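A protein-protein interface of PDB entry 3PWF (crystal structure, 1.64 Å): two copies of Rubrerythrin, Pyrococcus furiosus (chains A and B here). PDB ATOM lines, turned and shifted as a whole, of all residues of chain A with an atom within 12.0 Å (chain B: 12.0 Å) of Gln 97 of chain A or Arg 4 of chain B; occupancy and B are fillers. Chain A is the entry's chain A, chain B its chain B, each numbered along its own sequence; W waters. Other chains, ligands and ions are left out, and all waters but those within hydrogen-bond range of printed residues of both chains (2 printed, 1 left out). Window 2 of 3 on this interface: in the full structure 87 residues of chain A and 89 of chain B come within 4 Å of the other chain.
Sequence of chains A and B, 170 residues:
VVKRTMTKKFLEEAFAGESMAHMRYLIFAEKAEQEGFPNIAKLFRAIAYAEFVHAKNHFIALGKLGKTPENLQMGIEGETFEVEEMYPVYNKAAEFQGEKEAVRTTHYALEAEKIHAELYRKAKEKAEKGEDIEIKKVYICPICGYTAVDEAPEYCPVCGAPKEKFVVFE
OE1 of Glu 13 of chain B is in hydrogen-bond range of OH of Tyr 90 of chain A (2.6 Å).
The side-chain amide oxygen (OE1) of Gln 97 of chain A is in hydrogen-bond range of the side-chain hydroxyl (OG1) of Thr 7 of chain B.
The backbone NH of Lys 3 of chain B is in hydrogen-bond range of the side-chain carboxylate of Glu 99 of chain A (2.8 Å).
The backbone NH of Arg 4 of chain B is in hydrogen-bond range of the side-chain carboxylate of Glu 99 of chain A, at 2.9 Å.
N of Val 1 of chain B sits at hydrogen-bond distance from OE1 of Glu 101 of chain A, 2.7 Å away.
OG1 of Thr 105 of chain A lies within hydrogen-bond range of ND1 of His 58 of chain B.
The backbone carbonyl oxygen (O) of Ala 94 of chain A sits at hydrogen-bond distance from the backbone NH (N) of Glu 99 of chain A.
The backbone carbonyl oxygen (O) of Ala 61 of chain B sits at hydrogen-bond distance from the backbone NH (N) of Val 2 of chain B, 2.9 Å away.
NZ of Lys 9 of chain B is in salt-bridge range of OE2 of Glu 13 of chain B (3.9 Å).
Among the printed residues, merely in contact across the chains: Tyr 90 of chain A with Phe 10 of chain B (3.4 Å), Ala 93 of chain A with Thr 7 of chain B (3.96 Å), Ala 93 of chain A with Phe 10 of chain B (3.6 Å), Ala 94 of chain A with Thr 7 of chain B (3.6 Å), Gln 97 of chain A with Arg 4 of chain B (3.4 Å), Gln 97 of chain A with Met 6 of chain B (3.7 Å), Glu 99 of chain A with Val 2 of chain B (3.5 Å), Glu 99 of chain A with Thr 7 of chain B (3.9 Å), Glu 101 of chain A with Val 2 of chain B (3.8 Å), Glu 101 of chain A with Ala 61 of chain B (3.7 Å), Ala 102 of chain A with Thr 7 of chain B (3.4 Å), Ala 102 of chain A with Leu 11 of chain B (3.9 Å) and Thr 105 of chain A with Leu 11 of chain B (3.7 Å).
Of the printed residues of chain B, Tyr 90 of chain A touches Phe 10 (3.4 Å) and Glu 13 (2.6 Å).
Asn 91 of chain A touches none of the printed residues of chain B.
Ala 94 of chain A touches just one residue of chain B: Thr 7 (3.6 Å).
No residue of chain B comes within 4 Å of Phe 96 of chain A.
Of chain B, only Arg 4 (3.4 Å), Met 6 (3.7 Å) and Thr 7 (2.7 Å) come within 4 Å of Gln 97 of chain A.
No residue of chain B comes within 4 Å of Gly 98 of chain A.
Of the printed residues of chain A, Lys 3 of chain B touches Glu 99 (2.8 Å).
Of chain A, only Gln 97 and Glu 99 come within 4 Å of Arg 4 of chain B.
No residue of chain A comes within 4 Å of Thr 5 of chain B.
Of the printed residues of chain A, Thr 7 of chain B touches Ala 93, Ala 94, Gln 97, Glu 99 and Ala 102.
The nearest residue of chain B that does not touch Gln 97 of chain A is Thr 5 of chain B (4.8 Å).
The nearest residue of chain A that does not touch Arg 4 of chain B is Gly 98 of chain A (6.0 Å).
Of the 18 printed residues of chain B, 11 touch a printed residue of chain A.
Hydrophobic or aromatic side chains of chain A within 4 Å of the printed part of chain B: Tyr 90, Ala 93 and Ala 102.
Among the printed residues, no Asp or Glu carboxylate lies within 4 Å of a Lys or Arg side-chain nitrogen of the other chain.
No position is printed for both chains.
Of the 19 pairs that touch across the chains among the printed residues, none has its exchanged pair printed and touching as well.
Water W2 bridges the side-chain carboxylate of Glu 99 of chain A and the side-chain amino group of Lys 3 of chain B.
Water W1 bridges OE2 of Glu 99 of chain A (2.8 Å) and O of Val 1 of chain B (2.8 Å).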
ATOM      1  N   PRO A  88       1.683   0.406  -7.788  1.00  0.00           N
ATOM      2  CA  PRO A  88       1.307  -0.651  -6.821  1.00  0.00           C
ATOM      3  C   PRO A  88       2.277  -1.848  -6.803  1.00  0.00           C
ATOM      4  O   PRO A  88       2.612  -2.326  -5.730  1.00  0.00           O
ATOM      5  CB  PRO A  88      -0.054  -1.132  -7.370  1.00  0.00           C
ATOM      6  CG  PRO A  88      -0.695   0.132  -7.880  1.00  0.00           C
ATOM      7  CD  PRO A  88       0.570   0.781  -8.669  1.00  0.00           C
ATOM      8  N   VAL A  89       2.814  -2.230  -8.017  1.00  0.00           N
ATOM      9  CA  VAL A  89       3.748  -3.347  -8.064  1.00  0.00           C
ATOM     10  C   VAL A  89       5.096  -2.872  -7.476  1.00  0.00           C
ATOM     11  O   VAL A  89       5.663  -3.653  -6.716  1.00  0.00           O
ATOM     12  CB  VAL A  89       3.901  -3.779  -9.529  1.00  0.00           C
ATOM     13  CG1 VAL A  89       5.164  -4.662  -9.705  1.00  0.00           C
ATOM     14  CG2 VAL A  89       2.609  -4.516  -9.904  1.00  0.00           C
ATOM     15  N   TYR A  90       5.604  -1.698  -7.872  1.00  0.00           N
ATOM     16  CA  TYR A  90       6.902  -1.285  -7.283  1.00  0.00           C
ATOM     17  C   TYR A  90       6.796  -1.111  -5.760  1.00  0.00           C
ATOM     18  O   TYR A  90       7.762  -1.476  -5.067  1.00  0.00           O
ATOM     19  CB  TYR A  90       7.355   0.049  -7.912  1.00  0.00           C
ATOM     20  CG  TYR A  90       7.843  -0.065  -9.313  1.00  0.00           C
ATOM     21  CD1 TYR A  90       7.970  -1.283  -9.974  1.00  0.00           C
ATOM     22  CD2 TYR A  90       8.168   1.140  -9.961  1.00  0.00           C
ATOM     23  CE1 TYR A  90       8.491  -1.293 -11.378  1.00  0.00           C
ATOM     24  CE2 TYR A  90       8.660   1.156 -11.319  1.00  0.00           C
ATOM     25  CZ  TYR A  90       8.854  -0.081 -11.918  1.00  0.00           C
ATOM     26  OH  TYR A  90       9.263  -0.023 -13.242  1.00  0.00           O
ATOM     27  N   ASN A  91       5.654  -0.553  -5.274  1.00  0.00           N
ATOM     28  CA  ASN A  91       5.512  -0.385  -3.795  1.00  0.00           C
ATOM     29  C   ASN A  91       5.411  -1.780  -3.129  1.00  0.00           C
ATOM     30  O   ASN A  91       6.093  -1.965  -2.078  1.00  0.00           O
ATOM     31  CB  ASN A  91       4.239   0.426  -3.638  1.00  0.00           C
ATOM     32  CG  ASN A  91       3.826   0.567  -2.138  1.00  0.00           C
ATOM     33  OD1 ASN A  91       3.147  -0.350  -1.568  1.00  0.00           O
ATOM     34  ND2 ASN A  91       4.340   1.603  -1.459  1.00  0.00           N
ATOM     35  N   LYS A  92       4.703  -2.767  -3.720  1.00  0.00           N
ATOM     36  CA  LYS A  92       4.651  -4.089  -3.058  1.00  0.00           C
ATOM     37  C   LYS A  92       6.025  -4.728  -3.138  1.00  0.00           C
ATOM     38  O   LYS A  92       6.417  -5.412  -2.162  1.00  0.00           O
ATOM     39  CB  LYS A  92       3.673  -4.962  -3.880  1.00  0.00           C
ATOM     40  CG  LYS A  92       3.431  -6.411  -3.353  1.00  0.00           C
ATOM     41  CD  LYS A  92       2.916  -6.501  -1.939  1.00  0.00           C
ATOM     42  CE  LYS A  92       1.719  -5.688  -1.615  1.00  0.00           C
ATOM     43  NZ  LYS A  92       1.302  -5.873  -0.093  1.00  0.00           N
ATOM     44  N   ALA A  93       6.786  -4.568  -4.239  1.00  0.00           N
ATOM     45  CA  ALA A  93       8.128  -5.179  -4.280  1.00  0.00           C
ATOM     46  C   ALA A  93       9.026  -4.571  -3.239  1.00  0.00           C
ATOM     47  O   ALA A  93       9.798  -5.281  -2.598  1.00  0.00           O
ATOM     48  CB  ALA A  93       8.729  -5.014  -5.687  1.00  0.00           C
ATOM     49  N   ALA A  94       8.948  -3.257  -3.074  1.00  0.00           N
ATOM     50  CA  ALA A  94       9.830  -2.602  -2.042  1.00  0.00           C
ATOM     51  C   ALA A  94       9.419  -3.073  -0.670  1.00  0.00           C
ATOM     52  O   ALA A  94      10.310  -3.330   0.172  1.00  0.00           O
ATOM     53  CB  ALA A  94       9.566  -1.040  -2.120  1.00  0.00           C
ATOM     54  N   GLU A  95       8.136  -3.242  -0.415  1.00  0.00           N
ATOM     55  CA  GLU A  95       7.713  -3.750   0.907  1.00  0.00           C
ATOM     56  C   GLU A  95       8.264  -5.175   1.152  1.00  0.00           C
ATOM     57  O   GLU A  95       8.850  -5.468   2.248  1.00  0.00           O
ATOM     58  CB  GLU A  95       6.158  -3.783   0.915  1.00  0.00           C
ATOM     59  CG  GLU A  95       5.583  -4.373   2.263  1.00  0.00           C
ATOM     60  CD  GLU A  95       4.098  -4.629   1.978  1.00  0.00           C
ATOM     61  OE1 GLU A  95       3.378  -3.651   1.724  1.00  0.00           O
ATOM     62  OE2 GLU A  95       3.723  -5.800   1.776  1.00  0.00           O
ATOM     63  N   PHE A  96       8.180  -6.042   0.083  1.00  0.00           N
ATOM     64  CA  PHE A  96       8.578  -7.417   0.159  1.00  0.00           C
ATOM     65  C   PHE A  96      10.112  -7.463   0.416  1.00  0.00           C
ATOM     66  O   PHE A  96      10.594  -8.372   1.111  1.00  0.00           O
ATOM     67  CB  PHE A  96       8.192  -8.080  -1.214  1.00  0.00           C
ATOM     68  CG  PHE A  96       8.676  -9.473  -1.355  1.00  0.00           C
ATOM     69  CD1 PHE A  96       9.714  -9.717  -2.175  1.00  0.00           C
ATOM     70  CD2 PHE A  96       8.062 -10.532  -0.707  1.00  0.00           C
ATOM     71  CE1 PHE A  96      10.169 -11.009  -2.393  1.00  0.00           C
ATOM     72  CE2 PHE A  96       8.573 -11.859  -0.824  1.00  0.00           C
ATOM     73  CZ  PHE A  96       9.620 -12.093  -1.726  1.00  0.00           C
ATOM     74  N   GLN A  97      10.841  -6.509  -0.181  1.00  0.00           N
ATOM     75  CA  GLN A  97      12.305  -6.475  -0.013  1.00  0.00           C
ATOM     76  C   GLN A  97      12.759  -5.660   1.244  1.00  0.00           C
ATOM     77  O   GLN A  97      13.959  -5.565   1.499  1.00  0.00           O
ATOM     78  CB  GLN A  97      12.974  -5.868  -1.276  1.00  0.00           C
ATOM     79  CG  GLN A  97      12.770  -6.806  -2.477  1.00  0.00           C
ATOM     80  CD  GLN A  97      13.880  -6.659  -3.467  1.00  0.00           C
ATOM     81  OE1 GLN A  97      14.129  -5.525  -3.950  1.00  0.00           O
ATOM     82  NE2 GLN A  97      14.559  -7.734  -3.797  1.00  0.00           N
ATOM     83  N   GLY A  98      11.795  -5.098   1.945  1.00  0.00           N
ATOM     84  CA  GLY A  98      12.215  -4.393   3.222  1.00  0.00           C
ATOM     85  C   GLY A  98      12.734  -3.017   3.004  1.00  0.00           C
ATOM     86  O   GLY A  98      13.345  -2.462   3.902  1.00  0.00           O
ATOM     87  N   GLU A  99      12.578  -2.428   1.813  1.00  0.00           N
ATOM     88  CA  GLU A  99      13.222  -1.172   1.480  1.00  0.00           C
ATOM     89  C   GLU A  99      12.305  -0.006   1.838  1.00  0.00           C
ATOM     90  O   GLU A  99      11.451   0.418   1.009  1.00  0.00           O
ATOM     91  CB  GLU A  99      13.544  -1.137  -0.039  1.00  0.00           C
ATOM     92  CG  GLU A  99      14.776  -2.033  -0.369  1.00  0.00           C
ATOM     93  CD  GLU A  99      16.137  -1.376   0.117  1.00  0.00           C
ATOM     94  OE1 GLU A  99      17.139  -1.988  -0.216  1.00  0.00           O
ATOM     95  OE2 GLU A  99      16.197  -0.295   0.817  1.00  0.00           O
ATOM     96  N   LYS A 100      12.329   0.366   3.120  1.00  0.00           N
ATOM     97  CA  LYS A 100      11.335   1.362   3.584  1.00  0.00           C
ATOM     98  C   LYS A 100      11.357   2.672   2.864  1.00  0.00           C
ATOM     99  O   LYS A 100      10.290   3.284   2.732  1.00  0.00           O
ATOM    100  CB  LYS A 100      11.670   1.675   5.068  1.00  0.00           C
ATOM    101  CG  LYS A 100      11.630   0.442   5.957  1.00  0.00           C
ATOM    102  CD  LYS A 100      10.473  -0.488   5.836  1.00  0.00           C
ATOM    103  CE  LYS A 100      10.688  -1.725   6.784  1.00  0.00           C
ATOM    104  NZ  LYS A 100       9.539  -2.670   6.718  1.00  0.00           N
ATOM    105  N   GLU A 101      12.531   3.161   2.434  1.00  0.00           N
ATOM    106  CA  GLU A 101      12.617   4.460   1.760  1.00  0.00           C
ATOM    107  C   GLU A 101      11.843   4.369   0.412  1.00  0.00           C
ATOM    108  O   GLU A 101      11.155   5.307   0.051  1.00  0.00           O
ATOM    109  CB  GLU A 101      14.043   4.895   1.422  1.00  0.00           C
ATOM    110  CG  GLU A 101      14.903   5.209   2.634  1.00  0.00           C
ATOM    111  CD  GLU A 101      16.278   5.419   2.093  1.00  0.00           C
ATOM    112  OE1 GLU A 101      17.068   4.380   2.233  1.00  0.00           O
ATOM    113  OE2 GLU A 101      16.422   6.522   1.397  1.00  0.00           O
ATOM    114  N   ALA A 102      11.989   3.226  -0.249  1.00  0.00           N
ATOM    115  CA  ALA A 102      11.270   3.038  -1.553  1.00  0.00           C
ATOM    116  C   ALA A 102       9.819   2.829  -1.352  1.00  0.00           C
ATOM    117  O   ALA A 102       9.011   3.192  -2.220  1.00  0.00           O
ATOM    118  CB  ALA A 102      11.909   1.842  -2.346  1.00  0.00           C
ATOM    119  N   VAL A 103       9.426   2.152  -0.253  1.00  0.00           N
ATOM    120  CA  VAL A 103       7.963   2.101   0.049  1.00  0.00           C
ATOM    121  C   VAL A 103       7.430   3.513   0.132  1.00  0.00           C
ATOM    122  O   VAL A 103       6.339   3.808  -0.388  1.00  0.00           O
ATOM    123  CB  VAL A 103       7.717   1.325   1.366  1.00  0.00           C
ATOM    124  CG1 VAL A 103       6.222   1.400   1.839  1.00  0.00           C
ATOM    125  CG2 VAL A 103       8.115  -0.198   1.229  1.00  0.00           C
ATOM    126  N   ARG A 104       8.130   4.371   0.875  1.00  0.00           N
ATOM    127  CA  ARG A 104       7.722   5.791   1.007  1.00  0.00           C
ATOM    128  C   ARG A 104       7.672   6.546  -0.320  1.00  0.00           C
ATOM    129  O   ARG A 104       6.617   7.168  -0.602  1.00  0.00           O
ATOM    130  CB  ARG A 104       8.616   6.523   2.043  1.00  0.00           C
ATOM    131  CG  ARG A 104       8.161   7.986   2.193  1.00  0.00           C
ATOM    132  CD  ARG A 104       8.897   8.563   3.438  1.00  0.00           C
ATOM    133  NE  ARG A 104      10.213   8.888   3.013  1.00  0.00           N
ATOM    134  CZ  ARG A 104      11.357   8.289   3.391  1.00  0.00           C
ATOM    135  NH1 ARG A 104      11.411   7.257   4.266  1.00  0.00           N
ATOM    136  NH2 ARG A 104      12.480   8.756   2.865  1.00  0.00           N
ATOM    137  N   THR A 105       8.743   6.476  -1.154  1.00  0.00           N
ATOM    138  CA  THR A 105       8.726   7.328  -2.384  1.00  0.00           C
ATOM    139  C   THR A 105       7.674   6.809  -3.331  1.00  0.00           C
ATOM    140  O   THR A 105       7.064   7.669  -4.012  1.00  0.00           O
ATOM    141  CB  THR A 105      10.083   7.472  -3.062  1.00  0.00           C
ATOM    142  OG1 THR A 105      10.502   6.180  -3.583  1.00  0.00           O
ATOM    143  CG2 THR A 105      11.122   7.963  -2.037  1.00  0.00           C
ATOM    144  N   THR A 106       7.445   5.474  -3.373  1.00  0.00           N
ATOM    145  CA  THR A 106       6.414   4.991  -4.314  1.00  0.00           C
ATOM    146  C   THR A 106       5.019   5.326  -3.779  1.00  0.00           C
ATOM    147  O   THR A 106       4.095   5.554  -4.605  1.00  0.00           O
ATOM    148  CB  THR A 106       6.533   3.489  -4.541  1.00  0.00           C
ATOM    149  OG1 THR A 106       6.492   2.739  -3.339  1.00  0.00           O
ATOM    150  CG2 THR A 106       7.889   3.207  -5.307  1.00  0.00           C
ATOM    151  N   VAL B   1      19.705   4.636   1.998  1.00  0.00           N
ATOM    152  CA  VAL B   1      19.952   4.496   0.469  1.00  0.00           C
ATOM    153  C   VAL B   1      19.467   3.080   0.142  1.00  0.00           C
ATOM    154  O   VAL B   1      19.741   2.124   0.869  1.00  0.00           O
ATOM    155  CB  VAL B   1      21.384   4.628   0.033  1.00  0.00           C
ATOM    156  CG1 VAL B   1      21.633   4.259  -1.521  1.00  0.00           C
ATOM    157  CG2 VAL B   1      21.936   6.056   0.398  1.00  0.00           C
ATOM    158  N   VAL B   2      18.669   2.938  -0.924  1.00  0.00           N
ATOM    159  CA  VAL B   2      18.163   1.629  -1.282  1.00  0.00           C
ATOM    160  C   VAL B   2      19.271   0.748  -1.791  1.00  0.00           C
ATOM    161  O   VAL B   2      20.143   1.225  -2.550  1.00  0.00           O
ATOM    162  CB  VAL B   2      17.087   1.858  -2.426  1.00  0.00           C
ATOM    163  CG1 VAL B   2      16.689   0.527  -3.075  1.00  0.00           C
ATOM    164  CG2 VAL B   2      15.892   2.515  -1.783  1.00  0.00           C
ATOM    165  N   LYS B   3      19.289  -0.551  -1.394  1.00  0.00           N
ATOM    166  CA  LYS B   3      20.428  -1.403  -1.755  1.00  0.00           C
ATOM    167  C   LYS B   3      20.004  -2.649  -2.518  1.00  0.00           C
ATOM    168  O   LYS B   3      20.834  -3.169  -3.310  1.00  0.00           O
ATOM    169  CB  LYS B   3      21.095  -1.938  -0.493  1.00  0.00           C
ATOM    170  CG  LYS B   3      21.717  -0.843   0.374  1.00  0.00           C
ATOM    171  CD  LYS B   3      22.491  -1.445   1.586  1.00  0.00           C
ATOM    172  CE  LYS B   3      21.666  -1.888   2.937  1.00  0.00           C
ATOM    173  NZ  LYS B   3      21.371  -3.353   3.468  1.00  0.00           N
ATOM    174  N   ARG B   4      18.774  -3.127  -2.332  1.00  0.00           N
ATOM    175  CA  ARG B   4      18.398  -4.416  -2.951  1.00  0.00           C
ATOM    176  C   ARG B   4      18.246  -4.235  -4.467  1.00  0.00           C
ATOM    177  O   ARG B   4      17.767  -3.176  -4.927  1.00  0.00           O
ATOM    178  CB  ARG B   4      17.058  -4.956  -2.371  1.00  0.00           C
ATOM    179  CG  ARG B   4      17.052  -5.239  -0.887  1.00  0.00           C
ATOM    180  CD  ARG B   4      17.946  -6.331  -0.587  1.00  0.00           C
ATOM    181  NE  ARG B   4      17.333  -7.495  -1.196  1.00  0.00           N
ATOM    182  CZ  ARG B   4      17.352  -8.716  -0.691  1.00  0.00           C
ATOM    183  NH1 ARG B   4      16.682  -9.675  -1.376  1.00  0.00           N
ATOM    184  NH2 ARG B   4      18.027  -8.961   0.517  1.00  0.00           N
ATOM    185  N   THR B   5      18.726  -5.221  -5.247  1.00  0.00           N
ATOM    186  CA  THR B   5      18.883  -5.043  -6.678  1.00  0.00           C
ATOM    187  C   THR B   5      17.561  -4.759  -7.414  1.00  0.00           C
ATOM    188  O   THR B   5      17.514  -3.840  -8.241  1.00  0.00           O
ATOM    189  CB  THR B   5      19.499  -6.315  -7.308  1.00  0.00           C
ATOM    190  OG1 THR B   5      20.805  -6.527  -6.645  1.00  0.00           O
ATOM    191  CG2 THR B   5      19.702  -6.088  -8.746  1.00  0.00           C
ATOM    192  N   MET B   6      16.548  -5.517  -7.091  1.00  0.00           N
ATOM    193  CA  MET B   6      15.284  -5.264  -7.802  1.00  0.00           C
ATOM    194  C   MET B   6      14.645  -3.938  -7.443  1.00  0.00           C
ATOM    195  O   MET B   6      14.224  -3.199  -8.374  1.00  0.00           O
ATOM    196  CB  MET B   6      14.252  -6.378  -7.573  1.00  0.00           C
ATOM    197  CG  MET B   6      14.756  -7.780  -8.048  1.00  0.00           C
ATOM    198  SD  MET B   6      15.212  -7.861  -9.772  1.00  0.00           S
ATOM    199  CE  MET B   6      13.652  -7.665 -10.616  1.00  0.00           C
ATOM    200  N   THR B   7      14.590  -3.547  -6.182  1.00  0.00           N
ATOM    201  CA  THR B   7      13.961  -2.281  -5.815  1.00  0.00           C
ATOM    202  C   THR B   7      14.816  -1.140  -6.406  1.00  0.00           C
ATOM    203  O   THR B   7      14.248  -0.117  -6.842  1.00  0.00           O
ATOM    204  CB  THR B   7      13.851  -2.181  -4.270  1.00  0.00           C
ATOM    205  OG1 THR B   7      12.903  -3.160  -3.841  1.00  0.00           O
ATOM    206  CG2 THR B   7      13.350  -0.807  -3.882  1.00  0.00           C
ATOM    207  N   LYS B   8      16.166  -1.275  -6.415  1.00  0.00           N
ATOM    208  CA  LYS B   8      17.007  -0.239  -7.040  1.00  0.00           C
ATOM    209  C   LYS B   8      16.607  -0.111  -8.500  1.00  0.00           C
ATOM    210  O   LYS B   8      16.448   1.002  -9.018  1.00  0.00           O
ATOM    211  CB  LYS B   8      18.495  -0.668  -6.916  1.00  0.00           C
ATOM    212  CG  LYS B   8      19.399   0.220  -7.595  1.00  0.00           C
ATOM    213  CD  LYS B   8      20.910  -0.286  -7.355  1.00  0.00           C
ATOM    214  CE  LYS B   8      21.849   0.503  -8.221  1.00  0.00           C
ATOM    215  NZ  LYS B   8      23.299   0.109  -7.916  1.00  0.00           N
ATOM    216  N   LYS B   9      16.503  -1.227  -9.227  1.00  0.00           N
ATOM    217  CA  LYS B   9      16.152  -1.154 -10.631  1.00  0.00           C
ATOM    218  C   LYS B   9      14.760  -0.459 -10.826  1.00  0.00           C
ATOM    219  O   LYS B   9      14.632   0.350 -11.722  1.00  0.00           O
ATOM    220  CB  LYS B   9      16.051  -2.589 -11.181  1.00  0.00           C
ATOM    221  CG  LYS B   9      15.539  -2.696 -12.645  1.00  0.00           C
ATOM    222  CD  LYS B   9      15.408  -4.236 -12.983  1.00  0.00           C
ATOM    223  CE  LYS B   9      15.463  -4.505 -14.570  1.00  0.00           C
ATOM    224  NZ  LYS B   9      14.120  -4.148 -15.218  1.00  0.00           N
ATOM    225  N   PHE B  10      13.832  -0.768  -9.938  1.00  0.00           N
ATOM    226  CA  PHE B  10      12.491  -0.235 -10.129  1.00  0.00           C
ATOM    227  C   PHE B  10      12.561   1.258  -9.818  1.00  0.00           C
ATOM    228  O   PHE B  10      11.863   2.002 -10.474  1.00  0.00           O
ATOM    229  CB  PHE B  10      11.500  -0.933  -9.138  1.00  0.00           C
ATOM    230  CG  PHE B  10      11.245  -2.387  -9.500  1.00  0.00           C
ATOM    231  CD1 PHE B  10      10.642  -3.230  -8.576  1.00  0.00           C
ATOM    232  CD2 PHE B  10      11.543  -2.845 -10.760  1.00  0.00           C
ATOM    233  CE1 PHE B  10      10.357  -4.605  -8.897  1.00  0.00           C
ATOM    234  CE2 PHE B  10      11.270  -4.228 -11.080  1.00  0.00           C
ATOM    235  CZ  PHE B  10      10.668  -5.108 -10.124  1.00  0.00           C
ATOM    236  N   LEU B  11      13.332   1.719  -8.833  1.00  0.00           N
ATOM    237  CA  LEU B  11      13.333   3.173  -8.576  1.00  0.00           C
ATOM    238  C   LEU B  11      14.101   3.834  -9.742  1.00  0.00           C
ATOM    239  O   LEU B  11      13.781   5.021 -10.020  1.00  0.00           O
ATOM    240  CB  LEU B  11      14.157   3.496  -7.262  1.00  0.00           C
ATOM    241  CG  LEU B  11      13.394   3.288  -5.993  1.00  0.00           C
ATOM    242  CD1 LEU B  11      14.054   3.894  -4.813  1.00  0.00           C
ATOM    243  CD2 LEU B  11      11.971   3.803  -6.052  1.00  0.00           C
ATOM    244  N   GLU B  12      15.094   3.181 -10.364  1.00  0.00           N
ATOM    245  CA  GLU B  12      15.742   3.851 -11.553  1.00  0.00           C
ATOM    246  C   GLU B  12      14.691   3.953 -12.686  1.00  0.00           C
ATOM    247  O   GLU B  12      14.681   5.013 -13.349  1.00  0.00           O
ATOM    248  CB  GLU B  12      16.891   2.990 -12.057  1.00  0.00           C
ATOM    249  CG  GLU B  12      18.038   3.120 -11.035  1.00  0.00           C
ATOM    250  CD  GLU B  12      19.163   2.121 -11.239  1.00  0.00           C
ATOM    251  OE1 GLU B  12      20.169   2.171 -10.463  1.00  0.00           O
ATOM    252  OE2 GLU B  12      19.044   1.255 -12.106  1.00  0.00           O
ATOM    253  N   GLU B  13      13.844   2.941 -12.850  1.00  0.00           N
ATOM    254  CA  GLU B  13      12.787   2.999 -13.894  1.00  0.00           C
ATOM    255  C   GLU B  13      11.810   4.114 -13.515  1.00  0.00           C
ATOM    256  O   GLU B  13      11.304   4.855 -14.378  1.00  0.00           O
ATOM    257  CB  GLU B  13      12.089   1.678 -13.991  1.00  0.00           C
ATOM    258  CG  GLU B  13      12.910   0.664 -14.882  1.00  0.00           C
ATOM    259  CD  GLU B  13      12.107  -0.619 -15.040  1.00  0.00           C
ATOM    260  OE1 GLU B  13      11.530  -1.068 -14.043  1.00  0.00           O
ATOM    261  OE2 GLU B  13      11.943  -1.087 -16.177  1.00  0.00           O
ATOM    262  N   HIS B  58      12.881   9.807  -5.598  1.00  0.00           N
ATOM    263  CA  HIS B  58      13.496   8.522  -5.947  1.00  0.00           C
ATOM    264  C   HIS B  58      15.006   8.687  -6.092  1.00  0.00           C
ATOM    265  O   HIS B  58      15.743   7.761  -5.702  1.00  0.00           O
ATOM    266  CB  HIS B  58      12.984   8.012  -7.317  1.00  0.00           C
ATOM    267  CG  HIS B  58      11.479   7.779  -7.345  1.00  0.00           C
ATOM    268  ND1 HIS B  58      10.761   7.268  -6.284  1.00  0.00           N
ATOM    269  CD2 HIS B  58      10.591   7.958  -8.368  1.00  0.00           C
ATOM    270  CE1 HIS B  58       9.469   7.153  -6.640  1.00  0.00           C
ATOM    271  NE2 HIS B  58       9.336   7.627  -7.886  1.00  0.00           N
ATOM    272  N   ALA B  61      16.547   8.650  -2.760  1.00  0.00           N
ATOM    273  CA  ALA B  61      16.485   7.258  -2.252  1.00  0.00           C
ATOM    274  C   ALA B  61      17.512   6.376  -2.866  1.00  0.00           C
ATOM    275  O   ALA B  61      18.017   5.464  -2.182  1.00  0.00           O
ATOM    276  CB  ALA B  61      14.995   6.685  -2.495  1.00  0.00           C
ATOM    277  N   LEU B  62      17.876   6.631  -4.095  1.00  0.00           N
ATOM    278  CA  LEU B  62      18.968   5.875  -4.747  1.00  0.00           C
ATOM    279  C   LEU B  62      20.419   6.382  -4.314  1.00  0.00           C
ATOM    280  O   LEU B  62      21.400   5.757  -4.777  1.00  0.00           O
ATOM    281  CB  LEU B  62      18.872   6.052  -6.230  1.00  0.00           C
ATOM    282  CG  LEU B  62      17.660   5.242  -6.824  1.00  0.00           C
ATOM    283  CD1 LEU B  62      17.330   5.825  -8.300  1.00  0.00           C
ATOM    284  CD2 LEU B  62      17.978   3.673  -6.803  1.00  0.00           C
ATOM    285  N   GLY B  63      20.444   7.451  -3.538  1.00  0.00           N
ATOM    286  CA  GLY B  63      21.768   7.988  -3.031  1.00  0.00           C
ATOM    287  C   GLY B  63      22.529   8.797  -4.088  1.00  0.00           C
ATOM    288  O   GLY B  63      23.794   9.007  -3.961  1.00  0.00           O
ATOM    289  N   LYS B  64      21.867   9.355  -5.111  1.00  0.00           N
ATOM    290  CA  LYS B  64      22.543   9.934  -6.231  1.00  0.00           C
ATOM    291  C   LYS B  64      22.769  11.414  -6.095  1.00  0.00           C
ATOM    292  O   LYS B  64      23.501  12.005  -6.937  1.00  0.00           O
ATOM    293  CB  LYS B  64      21.776   9.635  -7.546  1.00  0.00           C
ATOM    294  CG  LYS B  64      21.852   8.155  -7.819  1.00  0.00           C
ATOM    295  CD  LYS B  64      21.163   7.715  -9.089  1.00  0.00           C
ATOM    296  CE  LYS B  64      21.735   6.339  -9.538  1.00  0.00           C
ATOM    297  NZ  LYS B  64      21.244   5.888 -10.856  1.00  0.00           N
HETATM  298  O   HOH W   1      18.413   0.192   2.448  1.00  0.00           O
HETATM  299  O   HOH W   2      18.190  -3.039   2.093  1.00  0.00           O
